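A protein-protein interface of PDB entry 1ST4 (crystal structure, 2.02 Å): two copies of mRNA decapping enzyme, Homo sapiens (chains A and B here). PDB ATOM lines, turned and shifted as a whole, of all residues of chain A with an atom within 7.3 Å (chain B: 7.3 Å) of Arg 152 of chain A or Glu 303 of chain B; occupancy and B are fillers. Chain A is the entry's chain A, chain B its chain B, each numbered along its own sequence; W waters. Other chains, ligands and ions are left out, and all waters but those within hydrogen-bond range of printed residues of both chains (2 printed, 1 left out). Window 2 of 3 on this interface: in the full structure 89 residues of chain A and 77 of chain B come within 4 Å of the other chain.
OD1 of Asn 304 of chain B sits close to NH2 of Arg 315 of chain A (2.2 Å).
The side-chain carboxylate (OE2) of Glu 303 of chain B lies within salt-bridge range of the guanidinium group (NH1) of Arg 152 of chain A (2.8 Å).
OE1 of Glu 303 of chain B lies within salt-bridge range of NH1 of Arg 315 of chain A, at 3.8 Å.
O of Arg 315 of chain A sits at hydrogen-bond distance from NH2 of Arg 231 of chain A, 2.6 Å away.
The backbone carbonyl oxygen (O) of Glu 303 of chain B lies within hydrogen-bond range of the side-chain sulfur (SG) of Cys 307 of chain B, at 3.2 Å.
O of Arg 152 of chain A is in hydrogen-bond range of NE2 of Gln 335 of chain A (3.2 Å).
The backbone carbonyl oxygen (O) of Glu 300 of chain B sits at hydrogen-bond distance from the side-chain amide nitrogen (ND2) of Asn 304 of chain B.
The side-chain amide nitrogen (ND2) of Asn 304 of chain B sits at hydrogen-bond distance from the side-chain hydroxyl (OH) of Tyr 312 of chain B, at 2.8 Å.
The side-chain hydroxyl (OG1) of Thr 318 of chain A lies within hydrogen-bond range of the guanidinium group (NE) of Arg 152 of chain A.
Among the printed residues, pairs that only touch across the chains: Arg 152 of chain A with Ala 299 of chain B, Thr 316 of chain A with Glu 300 of chain B, Thr 316 of chain A with Glu 303 of chain B and Thr 318 of chain A with Leu 297 of chain B.
Arg 152 of chain A touches just these residues of chain B: Ala 299 and Glu 303.
Of chain A, only Arg 152, Arg 315 and Thr 316 come within 4 Å of Glu 303 of chain B.
Of the printed residues of chain A, Asn 304 of chain B touches Arg 315 (2.2 Å).
Printed residues of chain B within 4 Å of Arg 315 of chain A: Glu 303 and Asn 304.
Printed residues of chain B within 4 Å of Thr 318 of chain A: Leu 297 (3.8 Å).
Of the printed residues of chain A, Ala 299 of chain B touches Arg 152.
Printed residues of chain A within 4 Å of Glu 300 of chain B: Thr 316.
Thr 154 of chain A touches none of the printed residues of chain B.
Gln 335 of chain A touches none of the printed residues of chain B.
The nearest residue of chain B that does not touch Arg 152 of chain A is Glu 300 of chain B (4.3 Å).
The nearest printed residue of chain A that does not touch Ala 299 of chain B is Thr 318 of chain A (5.9 Å).
Hydrophobic or aromatic side chains of chain B within 4 Å of the printed part of chain A: Leu 297 and Ala 299.
Among the printed residues, Asp or Glu carboxylates within 4 Å of a Lys or Arg side-chain nitrogen of the other chain: Arg 152 of chain A with Glu 303 of chain B (2.8 Å) and Arg 315 of chain A with Glu 303 of chain B (3.8 Å).
No position is printed for both chains.
Water W1 lies within hydrogen-bond range of OE1 of Glu 300 of chain B, O of Thr 316 of chain A, OG1 of Thr 318 of chain A and NH2 of Arg 152 of chain A.
Water W2 lies within hydrogen-bond range of OE1 of Glu 300 of chain B (2.8 Å) and N of Thr 318 of chain A (3.1 Å).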
ATOM      1  N   LEU A 150      13.810  14.003 -11.575  1.00  0.00           N
ATOM      2  CA  LEU A 150      13.673  14.445 -12.947  1.00  0.00           C
ATOM      3  C   LEU A 150      12.458  15.286 -13.187  1.00  0.00           C
ATOM      4  O   LEU A 150      11.399  15.094 -12.545  1.00  0.00           O
ATOM      5  CB  LEU A 150      13.596  13.227 -13.834  1.00  0.00           C
ATOM      6  CG  LEU A 150      14.307  13.015 -15.182  1.00  0.00           C
ATOM      7  CD1 LEU A 150      15.302  14.045 -15.538  1.00  0.00           C
ATOM      8  CD2 LEU A 150      15.007  11.715 -15.037  1.00  0.00           C
ATOM      9  N   ILE A 151      12.568  16.225 -14.116  1.00  0.00           N
ATOM     10  CA  ILE A 151      11.407  17.036 -14.449  1.00  0.00           C
ATOM     11  C   ILE A 151      11.400  17.371 -15.935  1.00  0.00           C
ATOM     12  O   ILE A 151      12.480  17.585 -16.531  1.00  0.00           O
ATOM     13  CB  ILE A 151      11.323  18.297 -13.523  1.00  0.00           C
ATOM     14  CG1 ILE A 151       9.986  19.004 -13.685  1.00  0.00           C
ATOM     15  CG2 ILE A 151      12.482  19.315 -13.804  1.00  0.00           C
ATOM     16  CD1 ILE A 151       8.857  18.455 -12.793  1.00  0.00           C
ATOM     17  N   ARG A 152      10.228  17.379 -16.572  1.00  0.00           N
ATOM     18  CA  ARG A 152      10.174  17.726 -17.977  1.00  0.00           C
ATOM     19  C   ARG A 152       9.584  19.120 -18.208  1.00  0.00           C
ATOM     20  O   ARG A 152       8.407  19.359 -17.967  1.00  0.00           O
ATOM     21  CB  ARG A 152       9.462  16.602 -18.793  1.00  0.00           C
ATOM     22  CG  ARG A 152       9.873  15.169 -18.411  1.00  0.00           C
ATOM     23  CD  ARG A 152       9.677  14.011 -19.496  1.00  0.00           C
ATOM     24  NE  ARG A 152      10.258  14.385 -20.814  1.00  0.00           N
ATOM     25  CZ  ARG A 152       9.579  14.842 -21.857  1.00  0.00           C
ATOM     26  NH1 ARG A 152       8.285  14.959 -21.791  1.00  0.00           N
ATOM     27  NH2 ARG A 152      10.176  15.188 -22.989  1.00  0.00           N
ATOM     28  N   GLU A 153      10.361  20.055 -18.743  1.00  0.00           N
ATOM     29  CA  GLU A 153       9.937  21.421 -18.664  1.00  0.00           C
ATOM     30  C   GLU A 153       9.502  21.826 -20.035  1.00  0.00           C
ATOM     31  O   GLU A 153      10.313  21.821 -20.947  1.00  0.00           O
ATOM     32  CB  GLU A 153      11.051  22.314 -18.112  1.00  0.00           C
ATOM     33  CG  GLU A 153      10.768  23.809 -18.111  1.00  0.00           C
ATOM     34  CD  GLU A 153      12.023  24.659 -18.262  1.00  0.00           C
ATOM     35  OE1 GLU A 153      12.323  25.423 -17.319  1.00  0.00           O
ATOM     36  OE2 GLU A 153      12.713  24.595 -19.307  1.00  0.00           O
ATOM     37  N   THR A 154       8.214  22.155 -20.177  1.00  0.00           N
ATOM     38  CA  THR A 154       7.599  22.543 -21.459  1.00  0.00           C
ATOM     39  C   THR A 154       8.075  23.938 -21.743  1.00  0.00           C
ATOM     40  O   THR A 154       8.492  24.633 -20.836  1.00  0.00           O
ATOM     41  CB  THR A 154       6.015  22.501 -21.324  1.00  0.00           C
ATOM     42  OG1 THR A 154       5.539  23.436 -20.289  1.00  0.00           O
ATOM     43  CG2 THR A 154       5.557  21.131 -20.814  1.00  0.00           C
ATOM     44  N   GLY A 155       8.052  24.382 -22.975  1.00  0.00           N
ATOM     45  CA  GLY A 155       8.368  25.769 -23.247  1.00  0.00           C
ATOM     46  C   GLY A 155       7.570  26.689 -22.318  1.00  0.00           C
ATOM     47  O   GLY A 155       8.082  27.729 -21.869  1.00  0.00           O
ATOM     48  N   ASP A 157       5.925  25.977 -19.263  1.00  0.00           N
ATOM     49  CA  ASP A 157       6.506  25.904 -17.923  1.00  0.00           C
ATOM     50  C   ASP A 157       7.757  26.788 -17.762  1.00  0.00           C
ATOM     51  O   ASP A 157       8.068  27.270 -16.629  1.00  0.00           O
ATOM     52  CB  ASP A 157       6.935  24.487 -17.598  1.00  0.00           C
ATOM     53  CG  ASP A 157       5.773  23.544 -17.458  1.00  0.00           C
ATOM     54  OD1 ASP A 157       4.724  23.959 -16.877  1.00  0.00           O
ATOM     55  OD2 ASP A 157       5.828  22.361 -17.901  1.00  0.00           O
ATOM     56  N   ARG A 231      17.819  28.057 -23.426  1.00  0.00           N
ATOM     57  CA  ARG A 231      16.476  28.599 -23.807  1.00  0.00           C
ATOM     58  C   ARG A 231      16.479  29.910 -24.571  1.00  0.00           C
ATOM     59  O   ARG A 231      15.502  30.234 -25.261  1.00  0.00           O
ATOM     60  CB  ARG A 231      15.553  28.679 -22.625  1.00  0.00           C
ATOM     61  CG  ARG A 231      15.329  27.292 -22.141  1.00  0.00           C
ATOM     62  CD  ARG A 231      14.004  26.938 -21.735  1.00  0.00           C
ATOM     63  NE  ARG A 231      13.329  26.261 -22.776  1.00  0.00           N
ATOM     64  CZ  ARG A 231      12.619  25.149 -22.682  1.00  0.00           C
ATOM     65  NH1 ARG A 231      12.488  24.440 -21.573  1.00  0.00           N
ATOM     66  NH2 ARG A 231      12.026  24.729 -23.784  1.00  0.00           N
ATOM     67  N   GLN A 314      10.232  26.247 -28.042  1.00  0.00           N
ATOM     68  CA  GLN A 314       9.043  25.380 -28.105  1.00  0.00           C
ATOM     69  C   GLN A 314       9.130  24.028 -27.407  1.00  0.00           C
ATOM     70  O   GLN A 314       8.156  23.589 -26.783  1.00  0.00           O
ATOM     71  CB  GLN A 314       8.525  25.231 -29.573  1.00  0.00           C
ATOM     72  CG  GLN A 314       7.997  26.580 -30.118  1.00  0.00           C
ATOM     73  CD  GLN A 314       7.975  26.708 -31.647  1.00  0.00           C
ATOM     74  OE1 GLN A 314       7.349  27.638 -32.189  1.00  0.00           O
ATOM     75  NE2 GLN A 314       8.677  25.805 -32.342  1.00  0.00           N
ATOM     76  N   ARG A 315      10.265  23.345 -27.490  1.00  0.00           N
ATOM     77  CA  ARG A 315      10.279  21.951 -27.077  1.00  0.00           C
ATOM     78  C   ARG A 315      10.466  21.792 -25.604  1.00  0.00           C
ATOM     79  O   ARG A 315      10.840  22.720 -24.917  1.00  0.00           O
ATOM     80  CB  ARG A 315      11.343  21.168 -27.850  1.00  0.00           C
ATOM     81  CG  ARG A 315      10.845  20.887 -29.299  1.00  0.00           C
ATOM     82  CD  ARG A 315      10.037  19.645 -29.419  1.00  0.00           C
ATOM     83  NE  ARG A 315      10.737  18.784 -30.357  1.00  0.00           N
ATOM     84  CZ  ARG A 315      11.107  17.544 -30.102  1.00  0.00           C
ATOM     85  NH1 ARG A 315      10.850  16.964 -28.937  1.00  0.00           N
ATOM     86  NH2 ARG A 315      11.719  16.881 -31.046  1.00  0.00           N
ATOM     87  N   THR A 316      10.264  20.583 -25.126  1.00  0.00           N
ATOM     88  CA  THR A 316      10.380  20.274 -23.720  1.00  0.00           C
ATOM     89  C   THR A 316      11.793  19.737 -23.403  1.00  0.00           C
ATOM     90  O   THR A 316      12.284  18.844 -24.110  1.00  0.00           O
ATOM     91  CB  THR A 316       9.340  19.155 -23.455  1.00  0.00           C
ATOM     92  OG1 THR A 316       8.014  19.686 -23.660  1.00  0.00           O
ATOM     93  CG2 THR A 316       9.372  18.683 -22.004  1.00  0.00           C
ATOM     94  N   LEU A 317      12.389  20.228 -22.306  1.00  0.00           N
ATOM     95  CA  LEU A 317      13.755  19.878 -21.880  1.00  0.00           C
ATOM     96  C   LEU A 317      13.671  19.132 -20.551  1.00  0.00           C
ATOM     97  O   LEU A 317      12.933  19.572 -19.660  1.00  0.00           O
ATOM     98  CB  LEU A 317      14.590  21.168 -21.761  1.00  0.00           C
ATOM     99  CG  LEU A 317      14.870  21.907 -23.092  1.00  0.00           C
ATOM    100  CD1 LEU A 317      15.709  23.213 -22.898  1.00  0.00           C
ATOM    101  CD2 LEU A 317      15.395  21.045 -24.340  1.00  0.00           C
ATOM    102  N   THR A 318      14.360  17.999 -20.437  1.00  0.00           N
ATOM    103  CA  THR A 318      14.429  17.226 -19.227  1.00  0.00           C
ATOM    104  C   THR A 318      15.685  17.513 -18.432  1.00  0.00           C
ATOM    105  O   THR A 318      16.783  17.430 -18.969  1.00  0.00           O
ATOM    106  CB  THR A 318      14.393  15.720 -19.588  1.00  0.00           C
ATOM    107  OG1 THR A 318      13.292  15.461 -20.449  1.00  0.00           O
ATOM    108  CG2 THR A 318      14.042  14.888 -18.440  1.00  0.00           C
ATOM    109  N   PHE A 319      15.552  17.765 -17.125  1.00  0.00           N
ATOM    110  CA  PHE A 319      16.707  17.939 -16.243  1.00  0.00           C
ATOM    111  C   PHE A 319      16.329  17.474 -14.828  1.00  0.00           C
ATOM    112  O   PHE A 319      15.191  17.203 -14.593  1.00  0.00           O
ATOM    113  CB  PHE A 319      17.158  19.382 -16.306  1.00  0.00           C
ATOM    114  CG  PHE A 319      16.091  20.398 -15.903  1.00  0.00           C
ATOM    115  CD1 PHE A 319      15.862  20.700 -14.571  1.00  0.00           C
ATOM    116  CD2 PHE A 319      15.349  21.056 -16.834  1.00  0.00           C
ATOM    117  CE1 PHE A 319      14.910  21.604 -14.190  1.00  0.00           C
ATOM    118  CE2 PHE A 319      14.405  21.997 -16.457  1.00  0.00           C
ATOM    119  CZ  PHE A 319      14.191  22.284 -15.159  1.00  0.00           C
ATOM    120  N   LEU A 328      11.156  22.813  -8.130  1.00  0.00           N
ATOM    121  CA  LEU A 328      10.607  21.513  -8.492  1.00  0.00           C
ATOM    122  C   LEU A 328       9.097  21.494  -8.176  1.00  0.00           C
ATOM    123  O   LEU A 328       8.252  21.210  -9.059  1.00  0.00           O
ATOM    124  CB  LEU A 328      11.327  20.377  -7.745  1.00  0.00           C
ATOM    125  CG  LEU A 328      10.783  18.947  -7.993  1.00  0.00           C
ATOM    126  CD1 LEU A 328      10.780  18.516  -9.470  1.00  0.00           C
ATOM    127  CD2 LEU A 328      11.566  17.984  -7.213  1.00  0.00           C
ATOM    128  N   LEU A 331       7.131  23.510 -10.353  1.00  0.00           N
ATOM    129  CA  LEU A 331       6.922  22.883 -11.661  1.00  0.00           C
ATOM    130  C   LEU A 331       6.048  21.633 -11.558  1.00  0.00           C
ATOM    131  O   LEU A 331       5.240  21.384 -12.441  1.00  0.00           O
ATOM    132  CB  LEU A 331       8.248  22.548 -12.375  1.00  0.00           C
ATOM    133  CG  LEU A 331       9.111  23.708 -12.902  1.00  0.00           C
ATOM    134  CD1 LEU A 331      10.480  23.149 -13.109  1.00  0.00           C
ATOM    135  CD2 LEU A 331       8.597  24.308 -14.204  1.00  0.00           C
ATOM    136  N   GLN A 335       1.937  20.959 -13.580  1.00  0.00           N
ATOM    137  CA  GLN A 335       1.717  19.922 -14.577  1.00  0.00           C
ATOM    138  C   GLN A 335       0.852  18.747 -14.125  1.00  0.00           C
ATOM    139  O   GLN A 335       0.089  18.228 -14.935  1.00  0.00           O
ATOM    140  CB  GLN A 335       3.010  19.491 -15.302  1.00  0.00           C
ATOM    141  CG  GLN A 335       4.149  18.881 -14.433  1.00  0.00           C
ATOM    142  CD  GLN A 335       5.522  18.746 -15.185  1.00  0.00           C
ATOM    143  OE1 GLN A 335       6.235  17.762 -14.999  1.00  0.00           O
ATOM    144  NE2 GLN A 335       5.866  19.730 -16.014  1.00  0.00           N
ATOM    145  N   LEU B 238       5.228   4.336 -32.306  1.00  0.00           N
ATOM    146  CA  LEU B 238       4.780   5.143 -31.198  1.00  0.00           C
ATOM    147  C   LEU B 238       4.106   4.250 -30.133  1.00  0.00           C
ATOM    148  O   LEU B 238       4.439   4.415 -28.963  1.00  0.00           O
ATOM    149  CB  LEU B 238       3.979   6.394 -31.641  1.00  0.00           C
ATOM    150  CG  LEU B 238       4.763   7.655 -32.048  1.00  0.00           C
ATOM    151  CD1 LEU B 238       4.027   8.755 -32.798  1.00  0.00           C
ATOM    152  CD2 LEU B 238       5.539   8.284 -30.818  1.00  0.00           C
ATOM    153  N   ARG B 242       5.639   4.174 -26.142  1.00  0.00           N
ATOM    154  CA  ARG B 242       4.724   4.671 -25.116  1.00  0.00           C
ATOM    155  C   ARG B 242       4.543   3.550 -24.193  1.00  0.00           C
ATOM    156  O   ARG B 242       4.680   3.674 -22.941  1.00  0.00           O
ATOM    157  CB  ARG B 242       3.381   5.048 -25.724  1.00  0.00           C
ATOM    158  CG  ARG B 242       3.417   6.399 -26.462  1.00  0.00           C
ATOM    159  CD  ARG B 242       2.337   6.608 -27.412  1.00  0.00           C
ATOM    160  NE  ARG B 242       2.409   7.975 -27.904  1.00  0.00           N
ATOM    161  CZ  ARG B 242       1.883   8.394 -29.051  1.00  0.00           C
ATOM    162  NH1 ARG B 242       1.191   7.541 -29.820  1.00  0.00           N
ATOM    163  NH2 ARG B 242       2.008   9.666 -29.436  1.00  0.00           N
ATOM    164  N   LEU B 245       7.827   2.987 -21.818  1.00  0.00           N
ATOM    165  CA  LEU B 245       7.983   4.061 -20.854  1.00  0.00           C
ATOM    166  C   LEU B 245       6.989   3.917 -19.712  1.00  0.00           C
ATOM    167  O   LEU B 245       7.380   3.740 -18.527  1.00  0.00           O
ATOM    168  CB  LEU B 245       7.723   5.360 -21.559  1.00  0.00           C
ATOM    169  CG  LEU B 245       8.783   6.452 -21.276  1.00  0.00           C
ATOM    170  CD1 LEU B 245       8.084   7.769 -21.289  1.00  0.00           C
ATOM    171  CD2 LEU B 245       9.666   6.168 -19.971  1.00  0.00           C
ATOM    172  N   LEU B 297      17.054   9.897 -24.428  1.00  0.00           N
ATOM    173  CA  LEU B 297      15.936   9.704 -23.484  1.00  0.00           C
ATOM    174  C   LEU B 297      14.726   8.998 -24.184  1.00  0.00           C
ATOM    175  O   LEU B 297      14.322   9.463 -25.219  1.00  0.00           O
ATOM    176  CB  LEU B 297      15.553  11.028 -22.848  1.00  0.00           C
ATOM    177  CG  LEU B 297      16.512  11.332 -21.659  1.00  0.00           C
ATOM    178  CD1 LEU B 297      16.108  12.650 -21.067  1.00  0.00           C
ATOM    179  CD2 LEU B 297      16.621  10.239 -20.580  1.00  0.00           C
ATOM    180  N   LEU B 298      14.210   7.896 -23.670  1.00  0.00           N
ATOM    181  CA  LEU B 298      12.921   7.373 -24.284  1.00  0.00           C
ATOM    182  C   LEU B 298      11.820   8.415 -24.596  1.00  0.00           C
ATOM    183  O   LEU B 298      11.340   8.548 -25.744  1.00  0.00           O
ATOM    184  CB  LEU B 298      12.352   6.201 -23.473  1.00  0.00           C
ATOM    185  CG  LEU B 298      11.760   5.042 -24.366  1.00  0.00           C
ATOM    186  CD1 LEU B 298      10.762   4.223 -23.678  1.00  0.00           C
ATOM    187  CD2 LEU B 298      11.325   5.425 -25.873  1.00  0.00           C
ATOM    188  N   ALA B 299      11.489   9.269 -23.620  1.00  0.00           N
ATOM    189  CA  ALA B 299      10.440  10.239 -23.809  1.00  0.00           C
ATOM    190  C   ALA B 299      10.679  11.251 -24.859  1.00  0.00           C
ATOM    191  O   ALA B 299       9.691  11.752 -25.461  1.00  0.00           O
ATOM    192  CB  ALA B 299      10.089  10.963 -22.462  1.00  0.00           C
ATOM    193  N   GLU B 300      11.938  11.621 -25.120  1.00  0.00           N
ATOM    194  CA  GLU B 300      12.199  12.613 -26.192  1.00  0.00           C
ATOM    195  C   GLU B 300      12.269  11.923 -27.533  1.00  0.00           C
ATOM    196  O   GLU B 300      12.145  12.570 -28.548  1.00  0.00           O
ATOM    197  CB  GLU B 300      13.503  13.446 -26.043  1.00  0.00           C
ATOM    198  CG  GLU B 300      13.940  13.856 -24.640  1.00  0.00           C
ATOM    199  CD  GLU B 300      15.127  14.870 -24.668  1.00  0.00           C
ATOM    200  OE1 GLU B 300      14.890  16.052 -24.347  1.00  0.00           O
ATOM    201  OE2 GLU B 300      16.292  14.496 -25.008  1.00  0.00           O
ATOM    202  N   VAL B 301      12.595  10.658 -27.529  1.00  0.00           N
ATOM    203  CA  VAL B 301      12.511   9.869 -28.779  1.00  0.00           C
ATOM    204  C   VAL B 301      11.041   9.890 -29.181  1.00  0.00           C
ATOM    205  O   VAL B 301      10.711  10.414 -30.256  1.00  0.00           O
ATOM    206  CB  VAL B 301      13.036   8.431 -28.585  1.00  0.00           C
ATOM    207  CG1 VAL B 301      12.768   7.614 -29.846  1.00  0.00           C
ATOM    208  CG2 VAL B 301      14.557   8.442 -28.288  1.00  0.00           C
ATOM    209  N   ILE B 302      10.155   9.444 -28.279  1.00  0.00           N
ATOM    210  CA  ILE B 302       8.711   9.701 -28.491  1.00  0.00           C
ATOM    211  C   ILE B 302       8.361  11.110 -29.052  1.00  0.00           C
ATOM    212  O   ILE B 302       7.794  11.240 -30.203  1.00  0.00           O
ATOM    213  CB  ILE B 302       7.850   9.289 -27.256  1.00  0.00           C
ATOM    214  CG1 ILE B 302       7.871   7.781 -27.116  1.00  0.00           C
ATOM    215  CG2 ILE B 302       6.430   9.846 -27.422  1.00  0.00           C
ATOM    216  CD1 ILE B 302       7.847   7.187 -25.739  1.00  0.00           C
ATOM    217  N   GLU B 303       8.713  12.196 -28.345  1.00  0.00           N
ATOM    218  CA  GLU B 303       8.218  13.495 -28.845  1.00  0.00           C
ATOM    219  C   GLU B 303       8.867  13.865 -30.143  1.00  0.00           C
ATOM    220  O   GLU B 303       8.366  14.723 -30.903  1.00  0.00           O
ATOM    221  CB  GLU B 303       8.425  14.652 -27.869  1.00  0.00           C
ATOM    222  CG  GLU B 303       7.464  14.654 -26.709  1.00  0.00           C
ATOM    223  CD  GLU B 303       7.906  15.579 -25.602  1.00  0.00           C
ATOM    224  OE1 GLU B 303       8.679  16.535 -25.888  1.00  0.00           O
ATOM    225  OE2 GLU B 303       7.481  15.342 -24.439  1.00  0.00           O
ATOM    226  N   ASN B 304      10.045  13.308 -30.378  1.00  0.00           N
ATOM    227  CA  ASN B 304      10.741  13.612 -31.633  1.00  0.00           C
ATOM    228  C   ASN B 304       9.950  12.977 -32.837  1.00  0.00           C
ATOM    229  O   ASN B 304       9.813  13.587 -33.915  1.00  0.00           O
ATOM    230  CB  ASN B 304      12.142  12.991 -31.582  1.00  0.00           C
ATOM    231  CG  ASN B 304      13.197  13.950 -31.031  1.00  0.00           C
ATOM    232  OD1 ASN B 304      13.182  15.203 -31.246  1.00  0.00           O
ATOM    233  ND2 ASN B 304      14.183  13.356 -30.418  1.00  0.00           N
ATOM    234  N   LEU B 305       9.470  11.758 -32.620  1.00  0.00           N
ATOM    235  CA  LEU B 305       8.590  11.117 -33.609  1.00  0.00           C
ATOM    236  C   LEU B 305       7.363  11.992 -33.881  1.00  0.00           C
ATOM    237  O   LEU B 305       7.169  12.371 -35.007  1.00  0.00           O
ATOM    238  CB  LEU B 305       8.207   9.752 -33.112  1.00  0.00           C
ATOM    239  CG  LEU B 305       9.408   8.839 -33.272  1.00  0.00           C
ATOM    240  CD1 LEU B 305       9.160   7.529 -32.720  1.00  0.00           C
ATOM    241  CD2 LEU B 305       9.797   8.770 -34.762  1.00  0.00           C
ATOM    242  N   GLU B 306       6.698  12.451 -32.809  1.00  0.00           N
ATOM    243  CA  GLU B 306       5.526  13.270 -32.868  1.00  0.00           C
ATOM    244  C   GLU B 306       5.728  14.530 -33.676  1.00  0.00           C
ATOM    245  O   GLU B 306       4.759  15.028 -34.261  1.00  0.00           O
ATOM    246  CB  GLU B 306       4.967  13.639 -31.442  1.00  0.00           C
ATOM    247  CG  GLU B 306       4.444  12.445 -30.657  1.00  0.00           C
ATOM    248  CD  GLU B 306       4.203  12.689 -29.149  1.00  0.00           C
ATOM    249  OE1 GLU B 306       4.345  13.862 -28.645  1.00  0.00           O
ATOM    250  OE2 GLU B 306       3.915  11.645 -28.429  1.00  0.00           O
ATOM    251  N   CYS B 307       6.910  15.103 -33.714  1.00  0.00           N
ATOM    252  CA  CYS B 307       6.997  16.395 -34.400  1.00  0.00           C
ATOM    253  C   CYS B 307       7.809  16.389 -35.671  1.00  0.00           C
ATOM    254  O   CYS B 307       7.833  17.384 -36.387  1.00  0.00           O
ATOM    255  CB  CYS B 307       7.518  17.506 -33.438  1.00  0.00           C
ATOM    256  SG  CYS B 307       6.825  17.396 -31.732  1.00  0.00           S
ATOM    257  N   ASP B 308       8.488  15.290 -35.937  1.00  0.00           N
ATOM    258  CA  ASP B 308       9.431  15.192 -37.053  1.00  0.00           C
ATOM    259  C   ASP B 308       9.418  13.703 -37.446  1.00  0.00           C
ATOM    260  O   ASP B 308      10.372  13.003 -37.122  1.00  0.00           O
ATOM    261  CB  ASP B 308      10.832  15.657 -36.558  1.00  0.00           C
ATOM    262  CG  ASP B 308      11.921  15.810 -37.694  1.00  0.00           C
ATOM    263  OD1 ASP B 308      11.609  15.558 -38.871  1.00  0.00           O
ATOM    264  OD2 ASP B 308      13.141  16.158 -37.470  1.00  0.00           O
ATOM    265  N   TYR B 312      14.774  10.079 -37.174  1.00  0.00           N
ATOM    266  CA  TYR B 312      15.800   9.120 -37.044  1.00  0.00           C
ATOM    267  C   TYR B 312      16.370   8.451 -38.309  1.00  0.00           C
ATOM    268  O   TYR B 312      17.327   7.653 -38.202  1.00  0.00           O
ATOM    269  CB  TYR B 312      15.312   8.105 -36.058  1.00  0.00           C
ATOM    270  CG  TYR B 312      15.182   8.786 -34.726  1.00  0.00           C
ATOM    271  CD1 TYR B 312      13.926   8.992 -34.117  1.00  0.00           C
ATOM    272  CD2 TYR B 312      16.327   9.305 -34.071  1.00  0.00           C
ATOM    273  CE1 TYR B 312      13.837   9.639 -32.868  1.00  0.00           C
ATOM    274  CE2 TYR B 312      16.239   9.953 -32.834  1.00  0.00           C
ATOM    275  CZ  TYR B 312      14.990  10.127 -32.238  1.00  0.00           C
ATOM    276  OH  TYR B 312      14.901  10.745 -30.980  1.00  0.00           O
HETATM  277  O   HOH W   1      12.996  16.716 -22.917  1.00  0.00           O
HETATM  278  O   HOH W   2      16.472  17.625 -22.662  1.00  0.00           O
